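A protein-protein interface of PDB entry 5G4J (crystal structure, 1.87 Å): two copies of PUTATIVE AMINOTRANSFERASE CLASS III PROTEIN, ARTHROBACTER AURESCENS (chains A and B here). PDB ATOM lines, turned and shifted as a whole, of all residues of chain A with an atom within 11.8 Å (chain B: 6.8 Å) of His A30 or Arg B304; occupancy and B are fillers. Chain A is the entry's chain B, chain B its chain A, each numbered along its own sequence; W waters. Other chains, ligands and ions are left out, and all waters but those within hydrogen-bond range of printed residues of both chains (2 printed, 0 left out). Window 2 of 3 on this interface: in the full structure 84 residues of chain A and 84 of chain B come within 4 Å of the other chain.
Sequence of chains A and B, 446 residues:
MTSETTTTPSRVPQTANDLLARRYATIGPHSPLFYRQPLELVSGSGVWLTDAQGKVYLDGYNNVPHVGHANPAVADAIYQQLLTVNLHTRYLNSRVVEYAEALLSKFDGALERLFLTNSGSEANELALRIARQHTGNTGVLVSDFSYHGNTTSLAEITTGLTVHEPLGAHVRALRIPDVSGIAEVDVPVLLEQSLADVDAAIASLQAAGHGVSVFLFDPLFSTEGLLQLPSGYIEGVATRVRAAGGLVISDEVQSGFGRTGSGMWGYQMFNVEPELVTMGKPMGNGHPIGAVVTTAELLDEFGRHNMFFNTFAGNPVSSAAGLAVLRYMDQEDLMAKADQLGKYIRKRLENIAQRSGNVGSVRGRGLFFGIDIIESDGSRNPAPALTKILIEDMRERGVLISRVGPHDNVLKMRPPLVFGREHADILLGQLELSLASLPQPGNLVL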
ATOM      1  N   LEU A  19       8.209   0.168  13.957  1.00  0.00           N
ATOM      2  CA  LEU A  19       9.391   1.043  13.703  1.00  0.00           C
ATOM      3  C   LEU A  19      10.361   0.500  12.632  1.00  0.00           C
ATOM      4  O   LEU A  19      10.771   1.248  11.700  1.00  0.00           O
ATOM      5  CB  LEU A  19      10.164   1.383  14.976  1.00  0.00           C
ATOM      6  CG  LEU A  19      11.200   2.497  14.773  1.00  0.00           C
ATOM      7  CD1 LEU A  19      10.544   3.822  14.415  1.00  0.00           C
ATOM      8  CD2 LEU A  19      12.026   2.662  16.023  1.00  0.00           C
ATOM      9  N   LEU A  20      10.691  -0.786  12.756  1.00  0.00           N
ATOM     10  CA  LEU A  20      11.531  -1.493  11.774  1.00  0.00           C
ATOM     11  C   LEU A  20      10.957  -1.343  10.349  1.00  0.00           C
ATOM     12  O   LEU A  20      11.688  -1.014   9.397  1.00  0.00           O
ATOM     13  CB  LEU A  20      11.732  -2.968  12.181  1.00  0.00           C
ATOM     14  CG  LEU A  20      12.857  -3.760  11.490  1.00  0.00           C
ATOM     15  CD1 LEU A  20      14.236  -3.073  11.636  1.00  0.00           C
ATOM     16  N   ALA A  21       9.646  -1.565  10.199  1.00  0.00           N
ATOM     17  CA  ALA A  21       9.035  -1.511   8.840  1.00  0.00           C
ATOM     18  C   ALA A  21       9.180  -0.112   8.266  1.00  0.00           C
ATOM     19  O   ALA A  21       9.456   0.059   7.078  1.00  0.00           O
ATOM     20  CB  ALA A  21       7.533  -1.898   8.857  1.00  0.00           C
ATOM     21  N   ARG A  22       8.857   0.873   9.119  1.00  0.00           N
ATOM     22  CA  ARG A  22       8.903   2.264   8.753  1.00  0.00           C
ATOM     23  C   ARG A  22      10.336   2.688   8.328  1.00  0.00           C
ATOM     24  O   ARG A  22      10.484   3.482   7.415  1.00  0.00           O
ATOM     25  CB  ARG A  22       8.402   3.151   9.920  1.00  0.00           C
ATOM     26  CG  ARG A  22       6.882   3.048  10.112  1.00  0.00           C
ATOM     27  CD  ARG A  22       6.428   3.634  11.447  1.00  0.00           C
ATOM     28  NE  ARG A  22       6.792   5.071  11.508  1.00  0.00           N
ATOM     29  CZ  ARG A  22       7.065   5.771  12.611  1.00  0.00           C
ATOM     30  NH1 ARG A  22       6.997   5.196  13.815  1.00  0.00           N
ATOM     31  NH2 ARG A  22       7.393   7.086  12.527  1.00  0.00           N
ATOM     32  N   ARG A  23      11.357   2.199   9.066  1.00  0.00           N
ATOM     33  CA  ARG A  23      12.733   2.424   8.704  1.00  0.00           C
ATOM     34  C   ARG A  23      13.032   1.834   7.322  1.00  0.00           C
ATOM     35  O   ARG A  23      13.639   2.473   6.449  1.00  0.00           O
ATOM     36  CB  ARG A  23      13.642   1.789   9.740  1.00  0.00           C
ATOM     37  CG  ARG A  23      15.133   1.891   9.365  1.00  0.00           C
ATOM     38  CD  ARG A  23      15.906   1.135  10.396  1.00  0.00           C
ATOM     39  NE  ARG A  23      17.306   0.919  10.029  1.00  0.00           N
ATOM     40  CZ  ARG A  23      18.348   1.432  10.683  1.00  0.00           C
ATOM     41  NH1 ARG A  23      18.159   2.220  11.764  1.00  0.00           N
ATOM     42  NH2 ARG A  23      19.593   1.165  10.258  1.00  0.00           N
ATOM     43  N   TYR A  24      12.630   0.588   7.116  1.00  0.00           N
ATOM     44  CA  TYR A  24      12.866  -0.113   5.825  1.00  0.00           C
ATOM     45  C   TYR A  24      12.186   0.570   4.600  1.00  0.00           C
ATOM     46  O   TYR A  24      12.745   0.594   3.501  1.00  0.00           O
ATOM     47  CB  TYR A  24      12.366  -1.596   5.966  1.00  0.00           C
ATOM     48  CG  TYR A  24      13.227  -2.547   6.765  1.00  0.00           C
ATOM     49  CD1 TYR A  24      14.404  -2.128   7.421  1.00  0.00           C
ATOM     50  CD2 TYR A  24      12.862  -3.911   6.875  1.00  0.00           C
ATOM     51  CE1 TYR A  24      15.194  -3.019   8.154  1.00  0.00           C
ATOM     52  CE2 TYR A  24      13.668  -4.821   7.602  1.00  0.00           C
ATOM     53  CZ  TYR A  24      14.813  -4.378   8.239  1.00  0.00           C
ATOM     54  OH  TYR A  24      15.586  -5.236   8.954  1.00  0.00           O
ATOM     55  N   ALA A  25      11.025   1.189   4.821  1.00  0.00           N
ATOM     56  CA  ALA A  25      10.305   1.966   3.807  1.00  0.00           C
ATOM     57  C   ALA A  25      10.984   3.330   3.451  1.00  0.00           C
ATOM     58  O   ALA A  25      10.588   3.983   2.461  1.00  0.00           O
ATOM     59  CB  ALA A  25       8.883   2.225   4.262  1.00  0.00           C
ATOM     60  N   THR A  26      11.964   3.780   4.256  1.00  0.00           N
ATOM     61  CA  THR A  26      12.550   5.134   4.079  1.00  0.00           C
ATOM     62  C   THR A  26      14.069   5.117   3.840  1.00  0.00           C
ATOM     63  O   THR A  26      14.594   5.478   2.767  1.00  0.00           O
ATOM     64  CB  THR A  26      12.181   6.048   5.282  1.00  0.00           C
ATOM     65  OG1 THR A  26      12.586   5.415   6.520  1.00  0.00           O
ATOM     66  CG2 THR A  26      10.662   6.373   5.239  1.00  0.00           C
ATOM     67  N   ILE A  27      14.789   4.671   4.837  1.00  0.00           N
ATOM     68  CA  ILE A  27      16.231   4.564   4.721  1.00  0.00           C
ATOM     69  C   ILE A  27      16.679   3.146   4.262  1.00  0.00           C
ATOM     70  O   ILE A  27      17.865   2.956   3.955  1.00  0.00           O
ATOM     71  CB  ILE A  27      16.984   5.050   5.989  1.00  0.00           C
ATOM     72  CG1 ILE A  27      16.708   4.200   7.186  1.00  0.00           C
ATOM     73  CG2 ILE A  27      16.590   6.492   6.321  1.00  0.00           C
ATOM     74  CD1 ILE A  27      17.659   4.490   8.353  1.00  0.00           C
ATOM     75  N   GLY A  28      15.729   2.194   4.179  1.00  0.00           N
ATOM     76  CA  GLY A  28      15.934   0.902   3.534  1.00  0.00           C
ATOM     77  C   GLY A  28      16.431  -0.150   4.506  1.00  0.00           C
ATOM     78  O   GLY A  28      16.821   0.178   5.676  1.00  0.00           O
ATOM     79  N   PRO A  29      16.467  -1.416   4.030  1.00  0.00           N
ATOM     80  CA  PRO A  29      16.774  -2.587   4.865  1.00  0.00           C
ATOM     81  C   PRO A  29      18.263  -2.926   4.934  1.00  0.00           C
ATOM     82  O   PRO A  29      18.637  -3.822   5.668  1.00  0.00           O
ATOM     83  CB  PRO A  29      16.022  -3.720   4.099  1.00  0.00           C
ATOM     84  CG  PRO A  29      16.239  -3.324   2.644  1.00  0.00           C
ATOM     85  CD  PRO A  29      16.060  -1.817   2.638  1.00  0.00           C
ATOM     86  N   HIS A  30      19.117  -2.234   4.160  1.00  0.00           N
ATOM     87  CA  HIS A  30      20.559  -2.571   4.114  1.00  0.00           C
ATOM     88  C   HIS A  30      21.343  -1.762   5.136  1.00  0.00           C
ATOM     89  O   HIS A  30      22.393  -2.197   5.611  1.00  0.00           O
ATOM     90  CB  HIS A  30      21.108  -2.332   2.708  1.00  0.00           C
ATOM     91  CG  HIS A  30      20.373  -3.100   1.648  1.00  0.00           C
ATOM     92  ND1 HIS A  30      20.409  -4.486   1.573  1.00  0.00           N
ATOM     93  CD2 HIS A  30      19.546  -2.688   0.655  1.00  0.00           C
ATOM     94  CE1 HIS A  30      19.653  -4.897   0.569  1.00  0.00           C
ATOM     95  NE2 HIS A  30      19.118  -3.828  -0.007  1.00  0.00           N
ATOM     96  N   SER A  31      20.858  -0.567   5.473  1.00  0.00           N
ATOM     97  CA  SER A  31      21.600   0.276   6.462  1.00  0.00           C
ATOM     98  C   SER A  31      21.803  -0.568   7.705  1.00  0.00           C
ATOM     99  O   SER A  31      20.825  -1.099   8.234  1.00  0.00           O
ATOM    100  CB  SER A  31      20.845   1.573   6.770  1.00  0.00           C
ATOM    101  OG  SER A  31      21.697   2.460   7.456  1.00  0.00           O
ATOM    102  N   PRO A  32      23.075  -0.788   8.139  1.00  0.00           N
ATOM    103  CA  PRO A  32      23.265  -1.896   9.128  1.00  0.00           C
ATOM    104  C   PRO A  32      22.542  -1.679  10.472  1.00  0.00           C
ATOM    105  O   PRO A  32      22.361  -0.491  10.904  1.00  0.00           O
ATOM    106  CB  PRO A  32      24.800  -1.913   9.376  1.00  0.00           C
ATOM    107  CG  PRO A  32      25.288  -0.549   8.876  1.00  0.00           C
ATOM    108  CD  PRO A  32      24.346  -0.168   7.742  1.00  0.00           C
ATOM    109  N   LEU A  33      22.161  -2.806  11.108  1.00  0.00           N
ATOM    110  CA  LEU A  33      21.618  -2.849  12.485  1.00  0.00           C
ATOM    111  C   LEU A  33      22.368  -3.953  13.246  1.00  0.00           C
ATOM    112  O   LEU A  33      22.636  -5.040  12.647  1.00  0.00           O
ATOM    113  CB  LEU A  33      20.111  -3.157  12.461  1.00  0.00           C
ATOM    114  CG  LEU A  33      19.182  -2.013  12.061  1.00  0.00           C
ATOM    115  CD1 LEU A  33      17.798  -2.533  11.642  1.00  0.00           C
ATOM    116  CD2 LEU A  33      19.074  -0.963  13.149  1.00  0.00           C
ATOM    117  N   PHE A  34      22.706  -3.692  14.528  1.00  0.00           N
ATOM    118  CA  PHE A  34      23.352  -4.678  15.382  1.00  0.00           C
ATOM    119  C   PHE A  34      22.300  -5.689  15.866  1.00  0.00           C
ATOM    120  O   PHE A  34      21.108  -5.331  16.034  1.00  0.00           O
ATOM    121  CB  PHE A  34      24.012  -4.062  16.650  1.00  0.00           C
ATOM    122  CG  PHE A  34      25.300  -3.253  16.393  1.00  0.00           C
ATOM    123  CD1 PHE A  34      26.277  -3.669  15.472  1.00  0.00           C
ATOM    124  CD2 PHE A  34      25.546  -2.086  17.137  1.00  0.00           C
ATOM    125  CE1 PHE A  34      27.466  -2.924  15.290  1.00  0.00           C
ATOM    126  CE2 PHE A  34      26.712  -1.341  16.947  1.00  0.00           C
ATOM    127  CZ  PHE A  34      27.686  -1.767  16.033  1.00  0.00           C
ATOM    128  N   TYR A  35      22.799  -6.923  16.109  1.00  0.00           N
ATOM    129  CA  TYR A  35      22.076  -8.019  16.774  1.00  0.00           C
ATOM    130  C   TYR A  35      21.081  -8.730  15.870  1.00  0.00           C
ATOM    131  O   TYR A  35      20.581  -8.152  14.870  1.00  0.00           O
ATOM    132  CB  TYR A  35      21.382  -7.538  18.082  1.00  0.00           C
ATOM    133  CG  TYR A  35      22.353  -6.919  19.079  1.00  0.00           C
ATOM    134  CD1 TYR A  35      23.346  -7.699  19.650  1.00  0.00           C
ATOM    135  CD2 TYR A  35      22.292  -5.539  19.435  1.00  0.00           C
ATOM    136  CE1 TYR A  35      24.261  -7.142  20.527  1.00  0.00           C
ATOM    137  CE2 TYR A  35      23.204  -4.968  20.333  1.00  0.00           C
ATOM    138  CZ  TYR A  35      24.194  -5.782  20.890  1.00  0.00           C
ATOM    139  OH  TYR A  35      25.151  -5.317  21.820  1.00  0.00           O
ATOM    140  N   PRO A  38      17.043  -6.335  16.120  1.00  0.00           N
ATOM    141  CA  PRO A  38      17.501  -4.922  16.307  1.00  0.00           C
ATOM    142  C   PRO A  38      17.008  -4.297  17.636  1.00  0.00           C
ATOM    143  O   PRO A  38      15.853  -4.508  18.013  1.00  0.00           O
ATOM    144  CB  PRO A  38      16.916  -4.197  15.085  1.00  0.00           C
ATOM    145  CG  PRO A  38      16.737  -5.265  14.040  1.00  0.00           C
ATOM    146  CD  PRO A  38      16.505  -6.574  14.765  1.00  0.00           C
ATOM    147  N   LEU A 161      35.797  -4.076   4.518  1.00  0.00           N
ATOM    148  CA  LEU A 161      34.342  -4.124   4.364  1.00  0.00           C
ATOM    149  C   LEU A 161      34.068  -4.242   2.880  1.00  0.00           C
ATOM    150  O   LEU A 161      34.916  -3.886   2.038  1.00  0.00           O
ATOM    151  CB  LEU A 161      33.823  -2.830   5.092  1.00  0.00           C
ATOM    152  CG  LEU A 161      32.719  -1.881   4.819  1.00  0.00           C
ATOM    153  CD1 LEU A 161      32.505  -0.951   6.019  1.00  0.00           C
ATOM    154  CD2 LEU A 161      33.017  -1.138   3.537  1.00  0.00           C
ATOM    155  N   THR A 162      32.882  -4.744   2.542  1.00  0.00           N
ATOM    156  CA  THR A 162      32.498  -4.933   1.159  1.00  0.00           C
ATOM    157  C   THR A 162      32.086  -3.682   0.448  1.00  0.00           C
ATOM    158  O   THR A 162      31.169  -2.980   0.914  1.00  0.00           O
ATOM    159  CB  THR A 162      31.337  -5.926   1.125  1.00  0.00           C
ATOM    160  OG1 THR A 162      31.810  -7.096   1.765  1.00  0.00           O
ATOM    161  CG2 THR A 162      30.952  -6.289  -0.308  1.00  0.00           C
ATOM    162  N   VAL A 163      32.750  -3.394  -0.669  1.00  0.00           N
ATOM    163  CA  VAL A 163      32.322  -2.292  -1.535  1.00  0.00           C
ATOM    164  C   VAL A 163      32.342  -2.807  -2.944  1.00  0.00           C
ATOM    165  O   VAL A 163      33.041  -3.754  -3.264  1.00  0.00           O
ATOM    166  CB  VAL A 163      33.241  -1.063  -1.419  1.00  0.00           C
ATOM    167  CG1 VAL A 163      33.193  -0.491  -0.008  1.00  0.00           C
ATOM    168  CG2 VAL A 163      34.651  -1.398  -1.801  1.00  0.00           C
ATOM    169  N   HIS A 164      31.605  -2.162  -3.810  1.00  0.00           N
ATOM    170  CA  HIS A 164      31.505  -2.583  -5.170  1.00  0.00           C
ATOM    171  C   HIS A 164      32.777  -2.255  -5.941  1.00  0.00           C
ATOM    172  O   HIS A 164      33.180  -2.977  -6.847  1.00  0.00           O
ATOM    173  CB  HIS A 164      30.340  -1.796  -5.790  1.00  0.00           C
ATOM    174  CG  HIS A 164      29.954  -2.253  -7.153  1.00  0.00           C
ATOM    175  ND1 HIS A 164      30.297  -1.570  -8.300  1.00  0.00           N
ATOM    176  CD2 HIS A 164      29.228  -3.312  -7.545  1.00  0.00           C
ATOM    177  CE1 HIS A 164      29.782  -2.189  -9.344  1.00  0.00           C
ATOM    178  NE2 HIS A 164      29.091  -3.226  -8.907  1.00  0.00           N
ATOM    179  N   GLU A 165      33.438  -1.153  -5.594  1.00  0.00           N
ATOM    180  CA  GLU A 165      34.650  -0.730  -6.316  1.00  0.00           C
ATOM    181  C   GLU A 165      35.774  -1.762  -6.122  1.00  0.00           C
ATOM    182  O   GLU A 165      36.068  -2.164  -4.969  1.00  0.00           O
ATOM    183  CB  GLU A 165      35.170   0.561  -5.726  1.00  0.00           C
ATOM    184  CG  GLU A 165      34.314   1.773  -6.015  1.00  0.00           C
ATOM    185  CD  GLU A 165      33.115   2.011  -5.105  1.00  0.00           C
ATOM    186  OE1 GLU A 165      32.795   1.170  -4.215  1.00  0.00           O
ATOM    187  OE2 GLU A 165      32.412   3.053  -5.320  1.00  0.00           O
ATOM    188  N   ALA B 296      13.486   3.652  -4.919  1.00  0.00           N
ATOM    189  CA  ALA B 296      13.634   2.356  -4.239  1.00  0.00           C
ATOM    190  C   ALA B 296      14.616   1.450  -4.946  1.00  0.00           C
ATOM    191  O   ALA B 296      15.430   0.772  -4.279  1.00  0.00           O
ATOM    192  CB  ALA B 296      12.241   1.640  -4.103  1.00  0.00           C
ATOM    193  N   GLU B 297      14.569   1.438  -6.274  1.00  0.00           N
ATOM    194  CA  GLU B 297      15.438   0.596  -7.046  1.00  0.00           C
ATOM    195  C   GLU B 297      16.915   0.994  -6.872  1.00  0.00           C
ATOM    196  O   GLU B 297      17.750   0.133  -6.633  1.00  0.00           O
ATOM    197  CB  GLU B 297      15.061   0.662  -8.506  1.00  0.00           C
ATOM    198  CG  GLU B 297      15.993  -0.175  -9.413  1.00  0.00           C
ATOM    199  N   LEU B 299      18.372   2.824  -4.288  1.00  0.00           N
ATOM    200  CA  LEU B 299      18.826   2.567  -2.903  1.00  0.00           C
ATOM    201  C   LEU B 299      19.024   1.049  -2.649  1.00  0.00           C
ATOM    202  O   LEU B 299      20.009   0.669  -2.007  1.00  0.00           O
ATOM    203  CB  LEU B 299      17.896   3.170  -1.859  1.00  0.00           C
ATOM    204  CG  LEU B 299      18.236   2.885  -0.381  1.00  0.00           C
ATOM    205  CD1 LEU B 299      18.063   4.133   0.480  1.00  0.00           C
ATOM    206  CD2 LEU B 299      17.467   1.674   0.162  1.00  0.00           C
ATOM    207  N   ASP B 300      18.077   0.235  -3.086  1.00  0.00           N
ATOM    208  CA  ASP B 300      18.172  -1.179  -2.864  1.00  0.00           C
ATOM    209  C   ASP B 300      19.447  -1.767  -3.531  1.00  0.00           C
ATOM    210  O   ASP B 300      20.176  -2.530  -2.893  1.00  0.00           O
ATOM    211  CB  ASP B 300      16.908  -1.942  -3.320  1.00  0.00           C
ATOM    212  CG  ASP B 300      17.008  -3.464  -2.987  1.00  0.00           C
ATOM    213  OD1 ASP B 300      16.975  -3.812  -1.778  1.00  0.00           O
ATOM    214  OD2 ASP B 300      17.221  -4.300  -3.908  1.00  0.00           O
ATOM    215  N   GLU B 301      19.706  -1.379  -4.785  1.00  0.00           N
ATOM    216  CA  GLU B 301      20.839  -1.853  -5.515  1.00  0.00           C
ATOM    217  C   GLU B 301      22.131  -1.455  -4.825  1.00  0.00           C
ATOM    218  O   GLU B 301      23.069  -2.274  -4.686  1.00  0.00           O
ATOM    219  CB  GLU B 301      20.811  -1.326  -6.945  1.00  0.00           C
ATOM    220  CG  GLU B 301      21.970  -1.731  -7.824  1.00  0.00           C
ATOM    221  CD  GLU B 301      21.901  -1.060  -9.159  1.00  0.00           C
ATOM    222  OE1 GLU B 301      21.448   0.084  -9.269  1.00  0.00           O
ATOM    223  OE2 GLU B 301      22.310  -1.644 -10.134  1.00  0.00           O
ATOM    224  N   PHE B 302      22.232  -0.175  -4.480  1.00  0.00           N
ATOM    225  CA  PHE B 302      23.444   0.291  -3.805  1.00  0.00           C
ATOM    226  C   PHE B 302      23.693  -0.411  -2.491  1.00  0.00           C
ATOM    227  O   PHE B 302      24.811  -0.846  -2.215  1.00  0.00           O
ATOM    228  CB  PHE B 302      23.421   1.813  -3.624  1.00  0.00           C
ATOM    229  CG  PHE B 302      24.742   2.407  -3.161  1.00  0.00           C
ATOM    230  CD1 PHE B 302      25.760   2.610  -4.036  1.00  0.00           C
ATOM    231  CD2 PHE B 302      24.908   2.765  -1.860  1.00  0.00           C
ATOM    232  CE1 PHE B 302      26.939   3.221  -3.639  1.00  0.00           C
ATOM    233  CE2 PHE B 302      26.103   3.302  -1.433  1.00  0.00           C
ATOM    234  CZ  PHE B 302      27.108   3.529  -2.320  1.00  0.00           C
ATOM    235  N   GLY B 303      22.654  -0.590  -1.700  1.00  0.00           N
ATOM    236  CA  GLY B 303      22.760  -1.351  -0.461  1.00  0.00           C
ATOM    237  C   GLY B 303      23.104  -2.826  -0.645  1.00  0.00           C
ATOM    238  O   GLY B 303      23.823  -3.382   0.170  1.00  0.00           O
ATOM    239  N   ARG B 304      22.671  -3.445  -1.729  1.00  0.00           N
ATOM    240  CA  ARG B 304      23.071  -4.882  -1.981  1.00  0.00           C
ATOM    241  C   ARG B 304      24.570  -4.972  -2.313  1.00  0.00           C
ATOM    242  O   ARG B 304      25.212  -5.964  -1.998  1.00  0.00           O
ATOM    243  CB  ARG B 304      22.280  -5.509  -3.123  1.00  0.00           C
ATOM    244  CG  ARG B 304      20.870  -5.876  -2.675  1.00  0.00           C
ATOM    245  CD  ARG B 304      20.008  -6.510  -3.774  1.00  0.00           C
ATOM    246  NE  ARG B 304      20.465  -6.218  -5.145  1.00  0.00           N
ATOM    247  CZ  ARG B 304      19.855  -5.460  -6.069  1.00  0.00           C
ATOM    248  NH1 ARG B 304      18.709  -4.822  -5.825  1.00  0.00           N
ATOM    249  NH2 ARG B 304      20.440  -5.308  -7.257  1.00  0.00           N
ATOM    250  N   HIS B 305      25.130  -3.914  -2.884  1.00  0.00           N
ATOM    251  CA  HIS B 305      26.497  -3.948  -3.425  1.00  0.00           C
ATOM    252  C   HIS B 305      27.562  -3.359  -2.491  1.00  0.00           C
ATOM    253  O   HIS B 305      28.750  -3.547  -2.748  1.00  0.00           O
ATOM    254  CB  HIS B 305      26.526  -3.196  -4.755  1.00  0.00           C
ATOM    255  CG  HIS B 305      25.812  -3.874  -5.856  1.00  0.00           C
ATOM    256  ND1 HIS B 305      25.514  -3.231  -7.044  1.00  0.00           N
ATOM    257  CD2 HIS B 305      25.391  -5.152  -5.994  1.00  0.00           C
ATOM    258  CE1 HIS B 305      24.915  -4.095  -7.855  1.00  0.00           C
ATOM    259  NE2 HIS B 305      24.817  -5.259  -7.233  1.00  0.00           N
ATOM    260  N   ASN B 306      27.143  -2.691  -1.411  1.00  0.00           N
ATOM    261  CA  ASN B 306      28.079  -1.973  -0.582  1.00  0.00           C
ATOM    262  C   ASN B 306      27.587  -2.034   0.827  1.00  0.00           C
ATOM    263  O   ASN B 306      26.421  -1.761   1.093  1.00  0.00           O
ATOM    264  CB  ASN B 306      28.146  -0.476  -0.961  1.00  0.00           C
ATOM    265  CG  ASN B 306      28.436  -0.243  -2.444  1.00  0.00           C
ATOM    266  OD1 ASN B 306      27.541  -0.148  -3.274  1.00  0.00           O
ATOM    267  ND2 ASN B 306      29.652  -0.166  -2.758  1.00  0.00           N
ATOM    268  N   MET B 307      28.494  -2.267   1.774  1.00  0.00           N
ATOM    269  CA  MET B 307      28.147  -2.126   3.187  1.00  0.00           C
ATOM    270  C   MET B 307      28.375  -0.631   3.525  1.00  0.00           C
ATOM    271  O   MET B 307      29.386  -0.207   4.105  1.00  0.00           O
ATOM    272  CB  MET B 307      29.012  -3.049   4.032  1.00  0.00           C
ATOM    273  CG  MET B 307      28.896  -2.813   5.542  1.00  0.00           C
ATOM    274  SD  MET B 307      27.219  -2.656   6.257  1.00  0.00           S
ATOM    275  CE  MET B 307      26.596  -4.295   5.865  1.00  0.00           C
ATOM    276  N   PHE B 308      27.393   0.186   3.145  1.00  0.00           N
ATOM    277  CA  PHE B 308      27.510   1.630   3.242  1.00  0.00           C
ATOM    278  C   PHE B 308      27.040   2.083   4.632  1.00  0.00           C
ATOM    279  O   PHE B 308      25.960   1.706   5.118  1.00  0.00           O
ATOM    280  CB  PHE B 308      26.654   2.320   2.152  1.00  0.00           C
ATOM    281  CG  PHE B 308      26.734   3.826   2.228  1.00  0.00           C
ATOM    282  CD1 PHE B 308      27.851   4.498   1.748  1.00  0.00           C
ATOM    283  CD2 PHE B 308      25.748   4.556   2.890  1.00  0.00           C
ATOM    284  CE1 PHE B 308      27.931   5.894   1.877  1.00  0.00           C
ATOM    285  CE2 PHE B 308      25.841   5.929   3.044  1.00  0.00           C
ATOM    286  CZ  PHE B 308      26.923   6.605   2.554  1.00  0.00           C
HETATM  287  O   HOH W   1      23.753   3.405   6.031  1.00  0.00           O
HETATM  288  O   HOH W   2      24.302  -0.176   3.656  1.00  0.00           O
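The backbone carbonyl oxygen of Phe B302 lies close to the side-chain amide oxygen of Asn B306 (3.0 Å). NH1 of Arg B304 lies within salt-bridge range of OD2 of Asp B300, 2.5 Å away. The backbone carbonyl oxygen (O) of Arg A23 is in hydrogen-bond range of the backbone NH (N) of Gly A28. The guanidinium group of Arg A23 is in hydrogen-bond range of the backbone carbonyl oxygen of Pro A32 (3.3 Å).
Among the printed residues, pairs that only touch across the chains: Ile A27 with Leu B299 (3.7 Å), Gly A28 with Leu B299 (3.8 Å), His A30 with Gly B303 (3.6 Å), His A30 with Arg B304 (3.6 Å), Pro A32 with Met B307 (3.9 Å), Pro A32 with Phe B308 (3.6 Å), Leu A161 with Met B307 (3.7 Å), Thr A162 with Asn B306 (3.6 Å), Val A163 with His B305 (3.7 Å), Val A163 with Asn B306 (3.6 Å) and Glu A165 with Asn B306 (3.7 Å).
No position is printed for both chains.
Water W1 bridges OG of Ser A31 (2.7 Å) and O of Phe B308 (2.9 Å). Water W2 bridges the backbone carbonyl oxygen of Phe B308 and the backbone carbonyl oxygen of His A30.
Of the 23 printed residues of chain A, 9 touch a printed residue of chain B. Hydrophobic or aromatic side chains of chain A within 4 Å of the printed part of chain B: His A30, Pro A32, Leu A161, Val A163 and His A164. Of the 12 printed residues of chain B, 8 touch a printed residue of chain A. Along chain B the printed residues that touch a printed residue of chain A span positions 299 to 308. Among the printed residues, no Asp or Glu carboxylate lies within 4 Å of a Lys or Arg side-chain nitrogen of the other chain.
Leu A20 touches none of the printed residues of chain B. Printed residues of chain B within 4 Å of Ile A27: Leu B299 (3.7 Å). Of the printed residues of chain B, Gly A28 touches Leu B299 (3.8 Å). His A30 touches just these residues of chain B: Asp B300 (2.8 Å), Gly B303 (3.6 Å) and Arg B304 (3.6 Å). Of the printed residues of chain B, Glu A165 touches Asn B306 (3.7 Å). No residue of chain A comes within 4 Å of Glu B297. Of chain A, only His A30 comes within 4 Å of Asp B300. No residue of chain A comes within 4 Å of Glu B301. Of chain A, only His A30 (3.6 Å) comes within 4 Å of Gly B303. Of chain A, only His A30 comes within 4 Å of Arg B304. Of chain A, only Thr A162, Val A163, His A164 and Glu A165 come within 4 Å of Asn B306. Met B307 touches just these residues of chain A: Pro A32 (3.9 Å), Leu A161 (3.7 Å) and Thr A162 (2.9 Å). The nearest printed residue of chain B that does not touch Thr A162 is His B305 (4.3 Å).
The backbone carbonyl oxygen (O) of His B305 is in hydrogen-bond range of the backbone NH (N) of His A164, 3.3 Å away. N of Met B307 is in hydrogen-bond range of O of Thr A162 (2.9 Å). A ring nitrogen (NE2) of His A30 is in hydrogen-bond range of the side-chain carboxylate of Asp B300. The side-chain amide nitrogen (ND2) of Asn B306 lies close to the backbone NH (N) of His A164, at 3.0 Å.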
